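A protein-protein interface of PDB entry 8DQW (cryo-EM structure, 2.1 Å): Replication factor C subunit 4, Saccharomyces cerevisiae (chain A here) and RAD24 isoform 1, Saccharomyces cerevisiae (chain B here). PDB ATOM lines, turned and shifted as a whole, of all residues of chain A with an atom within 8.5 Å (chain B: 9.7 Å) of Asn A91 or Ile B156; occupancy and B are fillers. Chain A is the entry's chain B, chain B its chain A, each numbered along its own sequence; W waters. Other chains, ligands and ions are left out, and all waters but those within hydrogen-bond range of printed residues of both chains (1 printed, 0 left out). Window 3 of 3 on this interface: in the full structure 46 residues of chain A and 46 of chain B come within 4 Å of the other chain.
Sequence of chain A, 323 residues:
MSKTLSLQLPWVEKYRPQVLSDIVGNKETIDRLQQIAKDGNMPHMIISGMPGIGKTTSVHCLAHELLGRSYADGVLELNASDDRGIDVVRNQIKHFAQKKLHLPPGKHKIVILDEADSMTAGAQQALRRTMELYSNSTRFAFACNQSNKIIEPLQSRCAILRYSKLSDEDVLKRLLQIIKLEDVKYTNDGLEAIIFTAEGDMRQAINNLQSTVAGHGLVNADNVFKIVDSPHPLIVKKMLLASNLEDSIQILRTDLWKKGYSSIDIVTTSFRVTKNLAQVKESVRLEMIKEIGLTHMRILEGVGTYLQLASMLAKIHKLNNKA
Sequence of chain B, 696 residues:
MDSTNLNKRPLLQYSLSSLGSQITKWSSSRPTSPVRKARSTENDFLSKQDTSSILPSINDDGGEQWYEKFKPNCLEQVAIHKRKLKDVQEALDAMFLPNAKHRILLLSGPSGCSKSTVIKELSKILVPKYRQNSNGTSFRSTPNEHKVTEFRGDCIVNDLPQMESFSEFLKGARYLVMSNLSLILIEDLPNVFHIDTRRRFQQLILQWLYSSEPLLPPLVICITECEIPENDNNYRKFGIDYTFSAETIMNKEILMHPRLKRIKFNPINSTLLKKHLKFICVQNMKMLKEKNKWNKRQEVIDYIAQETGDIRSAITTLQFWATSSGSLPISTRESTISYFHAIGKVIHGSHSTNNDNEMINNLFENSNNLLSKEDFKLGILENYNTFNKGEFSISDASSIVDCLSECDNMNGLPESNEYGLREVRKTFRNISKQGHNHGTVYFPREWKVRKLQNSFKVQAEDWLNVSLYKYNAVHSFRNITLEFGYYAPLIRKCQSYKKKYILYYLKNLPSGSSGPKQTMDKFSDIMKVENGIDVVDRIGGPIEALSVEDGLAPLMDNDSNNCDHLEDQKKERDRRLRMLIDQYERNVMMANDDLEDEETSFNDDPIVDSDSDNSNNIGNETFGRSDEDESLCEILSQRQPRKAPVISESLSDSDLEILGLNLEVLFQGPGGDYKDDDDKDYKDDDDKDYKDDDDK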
ATOM      1  N   LEU A  76     -15.336  18.796 -15.776  1.00  0.00           N
ATOM      2  CA  LEU A  76     -16.410  17.843 -15.506  1.00  0.00           C
ATOM      3  C   LEU A  76     -16.723  17.905 -14.016  1.00  0.00           C
ATOM      4  O   LEU A  76     -15.905  17.487 -13.192  1.00  0.00           O
ATOM      5  CB  LEU A  76     -16.016  16.427 -15.927  1.00  0.00           C
ATOM      6  CG  LEU A  76     -17.020  15.322 -15.574  1.00  0.00           C
ATOM      7  CD1 LEU A  76     -18.384  15.610 -16.184  1.00  0.00           C
ATOM      8  CD2 LEU A  76     -16.507  13.961 -16.021  1.00  0.00           C
ATOM      9  N   GLY A  85     -21.909   6.325  -9.321  1.00  0.00           N
ATOM     10  CA  GLY A  85     -21.588   4.947  -9.038  1.00  0.00           C
ATOM     11  C   GLY A  85     -20.418   4.458  -9.874  1.00  0.00           C
ATOM     12  O   GLY A  85     -19.765   5.203 -10.606  1.00  0.00           O
ATOM     13  N   ILE A  86     -20.159   3.154  -9.755  1.00  0.00           N
ATOM     14  CA  ILE A  86     -19.012   2.563 -10.437  1.00  0.00           C
ATOM     15  C   ILE A  86     -19.182   2.652 -11.949  1.00  0.00           C
ATOM     16  O   ILE A  86     -18.208   2.838 -12.686  1.00  0.00           O
ATOM     17  CB  ILE A  86     -18.804   1.108  -9.975  1.00  0.00           C
ATOM     18  CG1 ILE A  86     -17.452   0.586 -10.469  1.00  0.00           C
ATOM     19  CG2 ILE A  86     -19.936   0.216 -10.474  1.00  0.00           C
ATOM     20  CD1 ILE A  86     -16.990  -0.671  -9.766  1.00  0.00           C
ATOM     21  N   ASP A  87     -20.418   2.516 -12.436  1.00  0.00           N
ATOM     22  CA  ASP A  87     -20.654   2.627 -13.872  1.00  0.00           C
ATOM     23  C   ASP A  87     -20.315   4.023 -14.379  1.00  0.00           C
ATOM     24  O   ASP A  87     -19.808   4.182 -15.498  1.00  0.00           O
ATOM     25  CB  ASP A  87     -22.107   2.279 -14.194  1.00  0.00           C
ATOM     26  CG  ASP A  87     -22.339   2.071 -15.679  1.00  0.00           C
ATOM     27  OD1 ASP A  87     -22.790   3.022 -16.352  1.00  0.00           O
ATOM     28  OD2 ASP A  87     -22.070   0.955 -16.172  1.00  0.00           O
ATOM     29  N   VAL A  88     -20.593   5.049 -13.575  1.00  0.00           N
ATOM     30  CA  VAL A  88     -20.247   6.410 -13.970  1.00  0.00           C
ATOM     31  C   VAL A  88     -18.738   6.546 -14.126  1.00  0.00           C
ATOM     32  O   VAL A  88     -18.254   7.102 -15.117  1.00  0.00           O
ATOM     33  CB  VAL A  88     -20.813   7.423 -12.958  1.00  0.00           C
ATOM     34  CG1 VAL A  88     -20.439   8.846 -13.356  1.00  0.00           C
ATOM     35  CG2 VAL A  88     -22.326   7.274 -12.859  1.00  0.00           C
ATOM     36  N   VAL A  89     -17.971   6.015 -13.171  1.00  0.00           N
ATOM     37  CA  VAL A  89     -16.516   6.027 -13.299  1.00  0.00           C
ATOM     38  C   VAL A  89     -16.090   5.256 -14.541  1.00  0.00           C
ATOM     39  O   VAL A  89     -15.183   5.673 -15.271  1.00  0.00           O
ATOM     40  CB  VAL A  89     -15.860   5.454 -12.028  1.00  0.00           C
ATOM     41  CG1 VAL A  89     -14.342   5.475 -12.155  1.00  0.00           C
ATOM     42  CG2 VAL A  89     -16.307   6.228 -10.798  1.00  0.00           C
ATOM     43  N   ARG A  90     -16.741   4.122 -14.802  1.00  0.00           N
ATOM     44  CA  ARG A  90     -16.353   3.277 -15.924  1.00  0.00           C
ATOM     45  C   ARG A  90     -16.597   3.959 -17.266  1.00  0.00           C
ATOM     46  O   ARG A  90     -15.826   3.747 -18.208  1.00  0.00           O
ATOM     47  CB  ARG A  90     -17.113   1.950 -15.868  1.00  0.00           C
ATOM     48  CG  ARG A  90     -16.544   0.936 -14.883  1.00  0.00           C
ATOM     49  CD  ARG A  90     -16.998  -0.477 -15.219  1.00  0.00           C
ATOM     50  NE  ARG A  90     -17.046  -1.342 -14.045  1.00  0.00           N
ATOM     51  CZ  ARG A  90     -18.153  -1.691 -13.399  1.00  0.00           C
ATOM     52  NH1 ARG A  90     -19.345  -1.256 -13.776  1.00  0.00           N
ATOM     53  NH2 ARG A  90     -18.061  -2.499 -12.346  1.00  0.00           N
ATOM     54  N   ASN A  91     -17.655   4.763 -17.382  1.00  0.00           N
ATOM     55  CA  ASN A  91     -18.036   5.326 -18.674  1.00  0.00           C
ATOM     56  C   ASN A  91     -17.809   6.830 -18.769  1.00  0.00           C
ATOM     57  O   ASN A  91     -16.985   7.272 -19.571  1.00  0.00           O
ATOM     58  CB  ASN A  91     -19.509   5.000 -18.955  1.00  0.00           C
ATOM     59  CG  ASN A  91     -19.736   3.529 -19.235  1.00  0.00           C
ATOM     60  OD1 ASN A  91     -19.510   3.055 -20.349  1.00  0.00           O
ATOM     61  ND2 ASN A  91     -20.180   2.795 -18.223  1.00  0.00           N
ATOM     62  N   GLN A  92     -18.466   7.632 -17.930  1.00  0.00           N
ATOM     63  CA  GLN A  92     -18.472   9.076 -18.153  1.00  0.00           C
ATOM     64  C   GLN A  92     -17.120   9.692 -17.818  1.00  0.00           C
ATOM     65  O   GLN A  92     -16.533  10.414 -18.635  1.00  0.00           O
ATOM     66  CB  GLN A  92     -19.577   9.724 -17.318  1.00  0.00           C
ATOM     67  CG  GLN A  92     -19.829  11.186 -17.644  1.00  0.00           C
ATOM     68  CD  GLN A  92     -20.902  11.800 -16.764  1.00  0.00           C
ATOM     69  OE1 GLN A  92     -21.617  11.095 -16.052  1.00  0.00           O
ATOM     70  NE2 GLN A  92     -21.020  13.122 -16.810  1.00  0.00           N
ATOM     71  N   ILE A  93     -16.612   9.424 -16.614  1.00  0.00           N
ATOM     72  CA  ILE A  93     -15.322   9.975 -16.214  1.00  0.00           C
ATOM     73  C   ILE A  93     -14.217   9.437 -17.110  1.00  0.00           C
ATOM     74  O   ILE A  93     -13.300  10.171 -17.498  1.00  0.00           O
ATOM     75  CB  ILE A  93     -15.053   9.675 -14.727  1.00  0.00           C
ATOM     76  CG1 ILE A  93     -16.073  10.408 -13.851  1.00  0.00           C
ATOM     77  CG2 ILE A  93     -13.631  10.071 -14.347  1.00  0.00           C
ATOM     78  CD1 ILE A  93     -16.153   9.898 -12.429  1.00  0.00           C
ATOM     79  N   LYS A  94     -14.285   8.150 -17.455  1.00  0.00           N
ATOM     80  CA  LYS A  94     -13.271   7.564 -18.324  1.00  0.00           C
ATOM     81  C   LYS A  94     -13.263   8.233 -19.693  1.00  0.00           C
ATOM     82  O   LYS A  94     -12.195   8.554 -20.228  1.00  0.00           O
ATOM     83  CB  LYS A  94     -13.510   6.058 -18.458  1.00  0.00           C
ATOM     84  CG  LYS A  94     -12.649   5.361 -19.506  1.00  0.00           C
ATOM     85  CD  LYS A  94     -12.944   3.866 -19.547  1.00  0.00           C
ATOM     86  CE  LYS A  94     -12.163   3.161 -20.644  1.00  0.00           C
ATOM     87  NZ  LYS A  94     -10.693   3.275 -20.460  1.00  0.00           N
ATOM     88  N   HIS A  95     -14.443   8.460 -20.277  1.00  0.00           N
ATOM     89  CA  HIS A  95     -14.504   9.101 -21.587  1.00  0.00           C
ATOM     90  C   HIS A  95     -14.033  10.547 -21.516  1.00  0.00           C
ATOM     91  O   HIS A  95     -13.351  11.027 -22.428  1.00  0.00           O
ATOM     92  CB  HIS A  95     -15.925   9.019 -22.144  1.00  0.00           C
ATOM     93  CG  HIS A  95     -16.409   7.617 -22.353  1.00  0.00           C
ATOM     94  ND1 HIS A  95     -17.731   7.257 -22.209  1.00  0.00           N
ATOM     95  CD2 HIS A  95     -15.744   6.485 -22.682  1.00  0.00           C
ATOM     96  CE1 HIS A  95     -17.862   5.964 -22.448  1.00  0.00           C
ATOM     97  NE2 HIS A  95     -16.671   5.472 -22.737  1.00  0.00           N
ATOM     98  N   PHE A  96     -14.388  11.261 -20.443  1.00  0.00           N
ATOM     99  CA  PHE A  96     -13.904  12.629 -20.289  1.00  0.00           C
ATOM    100  C   PHE A  96     -12.385  12.665 -20.184  1.00  0.00           C
ATOM    101  O   PHE A  96     -11.732  13.513 -20.802  1.00  0.00           O
ATOM    102  CB  PHE A  96     -14.536  13.280 -19.059  1.00  0.00           C
ATOM    103  CG  PHE A  96     -14.046  14.677 -18.798  1.00  0.00           C
ATOM    104  CD1 PHE A  96     -14.376  15.714 -19.655  1.00  0.00           C
ATOM    105  CD2 PHE A  96     -13.243  14.950 -17.702  1.00  0.00           C
ATOM    106  CE1 PHE A  96     -13.922  17.000 -19.419  1.00  0.00           C
ATOM    107  CE2 PHE A  96     -12.786  16.235 -17.461  1.00  0.00           C
ATOM    108  CZ  PHE A  96     -13.127  17.260 -18.321  1.00  0.00           C
ATOM    109  N   ALA A  97     -11.805  11.746 -19.409  1.00  0.00           N
ATOM    110  CA  ALA A  97     -10.356  11.723 -19.248  1.00  0.00           C
ATOM    111  C   ALA A  97      -9.657  11.271 -20.523  1.00  0.00           C
ATOM    112  O   ALA A  97      -8.497  11.633 -20.752  1.00  0.00           O
ATOM    113  CB  ALA A  97      -9.972  10.813 -18.081  1.00  0.00           C
ATOM    114  N   GLN A  98     -10.336  10.481 -21.357  1.00  0.00           N
ATOM    115  CA  GLN A  98      -9.772  10.062 -22.634  1.00  0.00           C
ATOM    116  C   GLN A  98      -9.845  11.150 -23.696  1.00  0.00           C
ATOM    117  O   GLN A  98      -9.112  11.078 -24.688  1.00  0.00           O
ATOM    118  CB  GLN A  98     -10.497   8.815 -23.145  1.00  0.00           C
ATOM    119  CG  GLN A  98      -9.945   7.510 -22.605  1.00  0.00           C
ATOM    120  CD  GLN A  98     -10.806   6.316 -22.974  1.00  0.00           C
ATOM    121  OE1 GLN A  98     -12.009   6.450 -23.201  1.00  0.00           O
ATOM    122  NE2 GLN A  98     -10.192   5.142 -23.036  1.00  0.00           N
ATOM    123  N   PHE B 151      -4.553  -6.811 -15.739  1.00  0.00           N
ATOM    124  CA  PHE B 151      -6.001  -6.827 -15.891  1.00  0.00           C
ATOM    125  C   PHE B 151      -6.560  -5.419 -15.732  1.00  0.00           C
ATOM    126  O   PHE B 151      -6.165  -4.676 -14.829  1.00  0.00           O
ATOM    127  CB  PHE B 151      -6.635  -7.761 -14.860  1.00  0.00           C
ATOM    128  CG  PHE B 151      -8.134  -7.683 -14.813  1.00  0.00           C
ATOM    129  CD1 PHE B 151      -8.900  -8.139 -15.874  1.00  0.00           C
ATOM    130  CD2 PHE B 151      -8.779  -7.155 -13.706  1.00  0.00           C
ATOM    131  CE1 PHE B 151     -10.280  -8.069 -15.830  1.00  0.00           C
ATOM    132  CE2 PHE B 151     -10.157  -7.081 -13.657  1.00  0.00           C
ATOM    133  CZ  PHE B 151     -10.909  -7.539 -14.722  1.00  0.00           C
ATOM    134  N   ARG B 152      -7.489  -5.058 -16.614  1.00  0.00           N
ATOM    135  CA  ARG B 152      -8.096  -3.731 -16.630  1.00  0.00           C
ATOM    136  C   ARG B 152      -9.548  -3.861 -16.182  1.00  0.00           C
ATOM    137  O   ARG B 152     -10.368  -4.469 -16.878  1.00  0.00           O
ATOM    138  CB  ARG B 152      -7.995  -3.109 -18.021  1.00  0.00           C
ATOM    139  CG  ARG B 152      -8.613  -1.726 -18.127  1.00  0.00           C
ATOM    140  CD  ARG B 152      -7.759  -0.792 -18.969  1.00  0.00           C
ATOM    141  NE  ARG B 152      -7.889  -1.067 -20.394  1.00  0.00           N
ATOM    142  CZ  ARG B 152      -8.952  -0.762 -21.126  1.00  0.00           C
ATOM    143  NH1 ARG B 152     -10.007  -0.162 -20.598  1.00  0.00           N
ATOM    144  NH2 ARG B 152      -8.957  -1.067 -22.420  1.00  0.00           N
ATOM    145  N   GLY B 153      -9.863  -3.284 -15.018  1.00  0.00           N
ATOM    146  CA  GLY B 153     -11.182  -3.443 -14.435  1.00  0.00           C
ATOM    147  C   GLY B 153     -12.270  -2.597 -15.063  1.00  0.00           C
ATOM    148  O   GLY B 153     -13.450  -2.935 -14.929  1.00  0.00           O
ATOM    149  N   ASP B 154     -11.909  -1.509 -15.739  1.00  0.00           N
ATOM    150  CA  ASP B 154     -12.895  -0.616 -16.335  1.00  0.00           C
ATOM    151  C   ASP B 154     -13.199  -0.950 -17.791  1.00  0.00           C
ATOM    152  O   ASP B 154     -13.977  -0.229 -18.425  1.00  0.00           O
ATOM    153  CB  ASP B 154     -12.428   0.842 -16.222  1.00  0.00           C
ATOM    154  CG  ASP B 154     -11.249   1.156 -17.126  1.00  0.00           C
ATOM    155  OD1 ASP B 154     -10.639   0.214 -17.671  1.00  0.00           O
ATOM    156  OD2 ASP B 154     -10.931   2.353 -17.289  1.00  0.00           O
ATOM    157  N   CYS B 155     -12.615  -2.015 -18.332  1.00  0.00           N
ATOM    158  CA  CYS B 155     -12.884  -2.393 -19.712  1.00  0.00           C
ATOM    159  C   CYS B 155     -14.284  -2.983 -19.835  1.00  0.00           C
ATOM    160  O   CYS B 155     -14.680  -3.840 -19.040  1.00  0.00           O
ATOM    161  CB  CYS B 155     -11.842  -3.398 -20.198  1.00  0.00           C
ATOM    162  SG  CYS B 155     -11.915  -3.753 -21.971  1.00  0.00           S
ATOM    163  N   ILE B 156     -15.035  -2.517 -20.830  1.00  0.00           N
ATOM    164  CA  ILE B 156     -16.367  -3.029 -21.126  1.00  0.00           C
ATOM    165  C   ILE B 156     -16.415  -3.365 -22.609  1.00  0.00           C
ATOM    166  O   ILE B 156     -16.124  -2.508 -23.451  1.00  0.00           O
ATOM    167  CB  ILE B 156     -17.470  -2.019 -20.764  1.00  0.00           C
ATOM    168  CG1 ILE B 156     -17.672  -1.978 -19.248  1.00  0.00           C
ATOM    169  CG2 ILE B 156     -18.778  -2.384 -21.459  1.00  0.00           C
ATOM    170  CD1 ILE B 156     -18.404  -0.742 -18.764  1.00  0.00           C
ATOM    171  N   VAL B 157     -16.783  -4.603 -22.925  1.00  0.00           N
ATOM    172  CA  VAL B 157     -16.939  -5.045 -24.301  1.00  0.00           C
ATOM    173  C   VAL B 157     -18.411  -5.357 -24.547  1.00  0.00           C
ATOM    174  O   VAL B 157     -19.207  -5.500 -23.619  1.00  0.00           O
ATOM    175  CB  VAL B 157     -16.048  -6.260 -24.627  1.00  0.00           C
ATOM    176  CG1 VAL B 157     -14.597  -5.827 -24.774  1.00  0.00           C
ATOM    177  CG2 VAL B 157     -16.185  -7.325 -23.553  1.00  0.00           C
ATOM    178  N   ASN B 158     -18.770  -5.460 -25.827  1.00  0.00           N
ATOM    179  CA  ASN B 158     -20.179  -5.560 -26.196  1.00  0.00           C
ATOM    180  C   ASN B 158     -20.773  -6.905 -25.794  1.00  0.00           C
ATOM    181  O   ASN B 158     -21.874  -6.966 -25.234  1.00  0.00           O
ATOM    182  CB  ASN B 158     -20.339  -5.332 -27.699  1.00  0.00           C
ATOM    183  CG  ASN B 158     -21.131  -4.080 -28.018  1.00  0.00           C
ATOM    184  OD1 ASN B 158     -21.960  -3.638 -27.225  1.00  0.00           O
ATOM    185  ND2 ASN B 158     -20.876  -3.500 -29.183  1.00  0.00           N
ATOM    186  N   ASP B 159     -20.060  -7.997 -26.064  1.00  0.00           N
ATOM    187  CA  ASP B 159     -20.620  -9.346 -25.971  1.00  0.00           C
ATOM    188  C   ASP B 159     -20.166 -10.080 -24.716  1.00  0.00           C
ATOM    189  O   ASP B 159     -19.886 -11.281 -24.764  1.00  0.00           O
ATOM    190  CB  ASP B 159     -20.257 -10.145 -27.219  1.00  0.00           C
ATOM    191  CG  ASP B 159     -21.063 -11.422 -27.354  1.00  0.00           C
ATOM    192  OD1 ASP B 159     -22.044 -11.593 -26.599  1.00  0.00           O
ATOM    193  OD2 ASP B 159     -20.714 -12.256 -28.215  1.00  0.00           O
ATOM    194  N   LEU B 160     -20.075  -9.393 -23.574  1.00  0.00           N
ATOM    195  CA  LEU B 160     -19.638 -10.048 -22.351  1.00  0.00           C
ATOM    196  C   LEU B 160     -20.252  -9.388 -21.121  1.00  0.00           C
ATOM    197  O   LEU B 160     -20.097  -8.169 -20.949  1.00  0.00           O
ATOM    198  CB  LEU B 160     -18.113 -10.022 -22.242  1.00  0.00           C
ATOM    199  CG  LEU B 160     -17.390 -11.372 -22.261  1.00  0.00           C
ATOM    200  CD1 LEU B 160     -15.905 -11.179 -21.999  1.00  0.00           C
ATOM    201  CD2 LEU B 160     -17.989 -12.335 -21.245  1.00  0.00           C
ATOM    202  N   PRO B 161     -20.939 -10.142 -20.260  1.00  0.00           N
ATOM    203  CA  PRO B 161     -21.393  -9.565 -18.990  1.00  0.00           C
ATOM    204  C   PRO B 161     -20.210  -9.147 -18.129  1.00  0.00           C
ATOM    205  O   PRO B 161     -19.120  -9.714 -18.212  1.00  0.00           O
ATOM    206  CB  PRO B 161     -22.191 -10.703 -18.339  1.00  0.00           C
ATOM    207  CG  PRO B 161     -22.529 -11.630 -19.445  1.00  0.00           C
ATOM    208  CD  PRO B 161     -21.419 -11.523 -20.436  1.00  0.00           C
ATOM    209  N   GLN B 162     -20.441  -8.132 -17.294  1.00  0.00           N
ATOM    210  CA  GLN B 162     -19.356  -7.563 -16.500  1.00  0.00           C
ATOM    211  C   GLN B 162     -18.716  -8.616 -15.601  1.00  0.00           C
ATOM    212  O   GLN B 162     -17.486  -8.742 -15.550  1.00  0.00           O
ATOM    213  CB  GLN B 162     -19.879  -6.393 -15.667  1.00  0.00           C
ATOM    214  CG  GLN B 162     -18.798  -5.423 -15.221  1.00  0.00           C
ATOM    215  CD  GLN B 162     -18.320  -4.530 -16.347  1.00  0.00           C
ATOM    216  OE1 GLN B 162     -19.097  -3.769 -16.922  1.00  0.00           O
ATOM    217  NE2 GLN B 162     -17.035  -4.620 -16.670  1.00  0.00           N
ATOM    218  N   MET B 163     -19.538  -9.396 -14.896  1.00  0.00           N
ATOM    219  CA  MET B 163     -19.008 -10.349 -13.926  1.00  0.00           C
ATOM    220  C   MET B 163     -18.076 -11.369 -14.563  1.00  0.00           C
ATOM    221  O   MET B 163     -17.224 -11.932 -13.867  1.00  0.00           O
ATOM    222  CB  MET B 163     -20.152 -11.074 -13.216  1.00  0.00           C
ATOM    223  CG  MET B 163     -21.039 -10.167 -12.382  1.00  0.00           C
ATOM    224  SD  MET B 163     -21.866 -11.041 -11.040  1.00  0.00           S
ATOM    225  CE  MET B 163     -23.139 -11.925 -11.939  1.00  0.00           C
ATOM    226  N   SER B 165     -15.925 -10.686 -17.059  1.00  0.00           N
ATOM    227  CA  SER B 165     -14.758 -10.069 -17.685  1.00  0.00           C
ATOM    228  C   SER B 165     -13.467 -10.708 -17.187  1.00  0.00           C
ATOM    229  O   SER B 165     -12.645 -11.179 -17.983  1.00  0.00           O
ATOM    230  CB  SER B 165     -14.753  -8.564 -17.410  1.00  0.00           C
ATOM    231  OG  SER B 165     -13.672  -7.934 -18.073  1.00  0.00           O
HETATM  232  O   HOH W   1     -15.431  -3.431 -12.197  1.00  0.00           O
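The side-chain amide nitrogen of Asn A91 sits at hydrogen-bond distance from the backbone carbonyl oxygen of Asp A87.
The side-chain carboxylate (OD1) of Asp B154 is in salt-bridge range of the guanidinium group (NH1) of Arg B152, 3.0 Å away.
O of Asn A91 sits at hydrogen-bond distance from ND1 of His A95.
The backbone NH (N) of Lys A94 lies within hydrogen-bond range of the backbone carbonyl oxygen (O) of Val A89, 3.4 Å away.
NE2 of Gln A98 lies close to NZ of Lys A94, at 3.2 Å.
Printed residues of chain B that touch a printed residue of chain A: Arg B152, Asp B154 and Ile B156.
Along chain B the printed residues that touch a printed residue of chain A span positions 152 to 156.
Among the printed residues, 4 pairs touch across the chains.
Among the printed residues, Asp or Glu carboxylates within 4 Å of a Lys or Arg side-chain nitrogen of the other chain: Lys A94 with Asp B154.
Of the printed residues of chain B, Asn A91 touches Ile B156.
Of the printed residues of chain A, Ile B156 touches Arg A90 (3.8 Å) and Asn A91 (3.99 Å).
No residue of chain A comes within 4 Å of Val B157.
Of the printed residues of chain B, Arg A90 touches Ile B156.
Of the printed residues of chain A, Asp B154 touches Lys A94.
The nearest printed residue of chain B that does not touch Asn A91 is Asp B154 (6.3 Å).
Water W1 bridges NH2 of Arg A90 (2.8 Å) and O of Gly B153 (3.4 Å).
NZ of Lys A94 is in salt-bridge range of OD2 of Asp B154, 3.3 Å away.
Ile B156 touches Arg A90.
Asn A91 touches Ile B156.
Lys A94 touches Arg B152.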
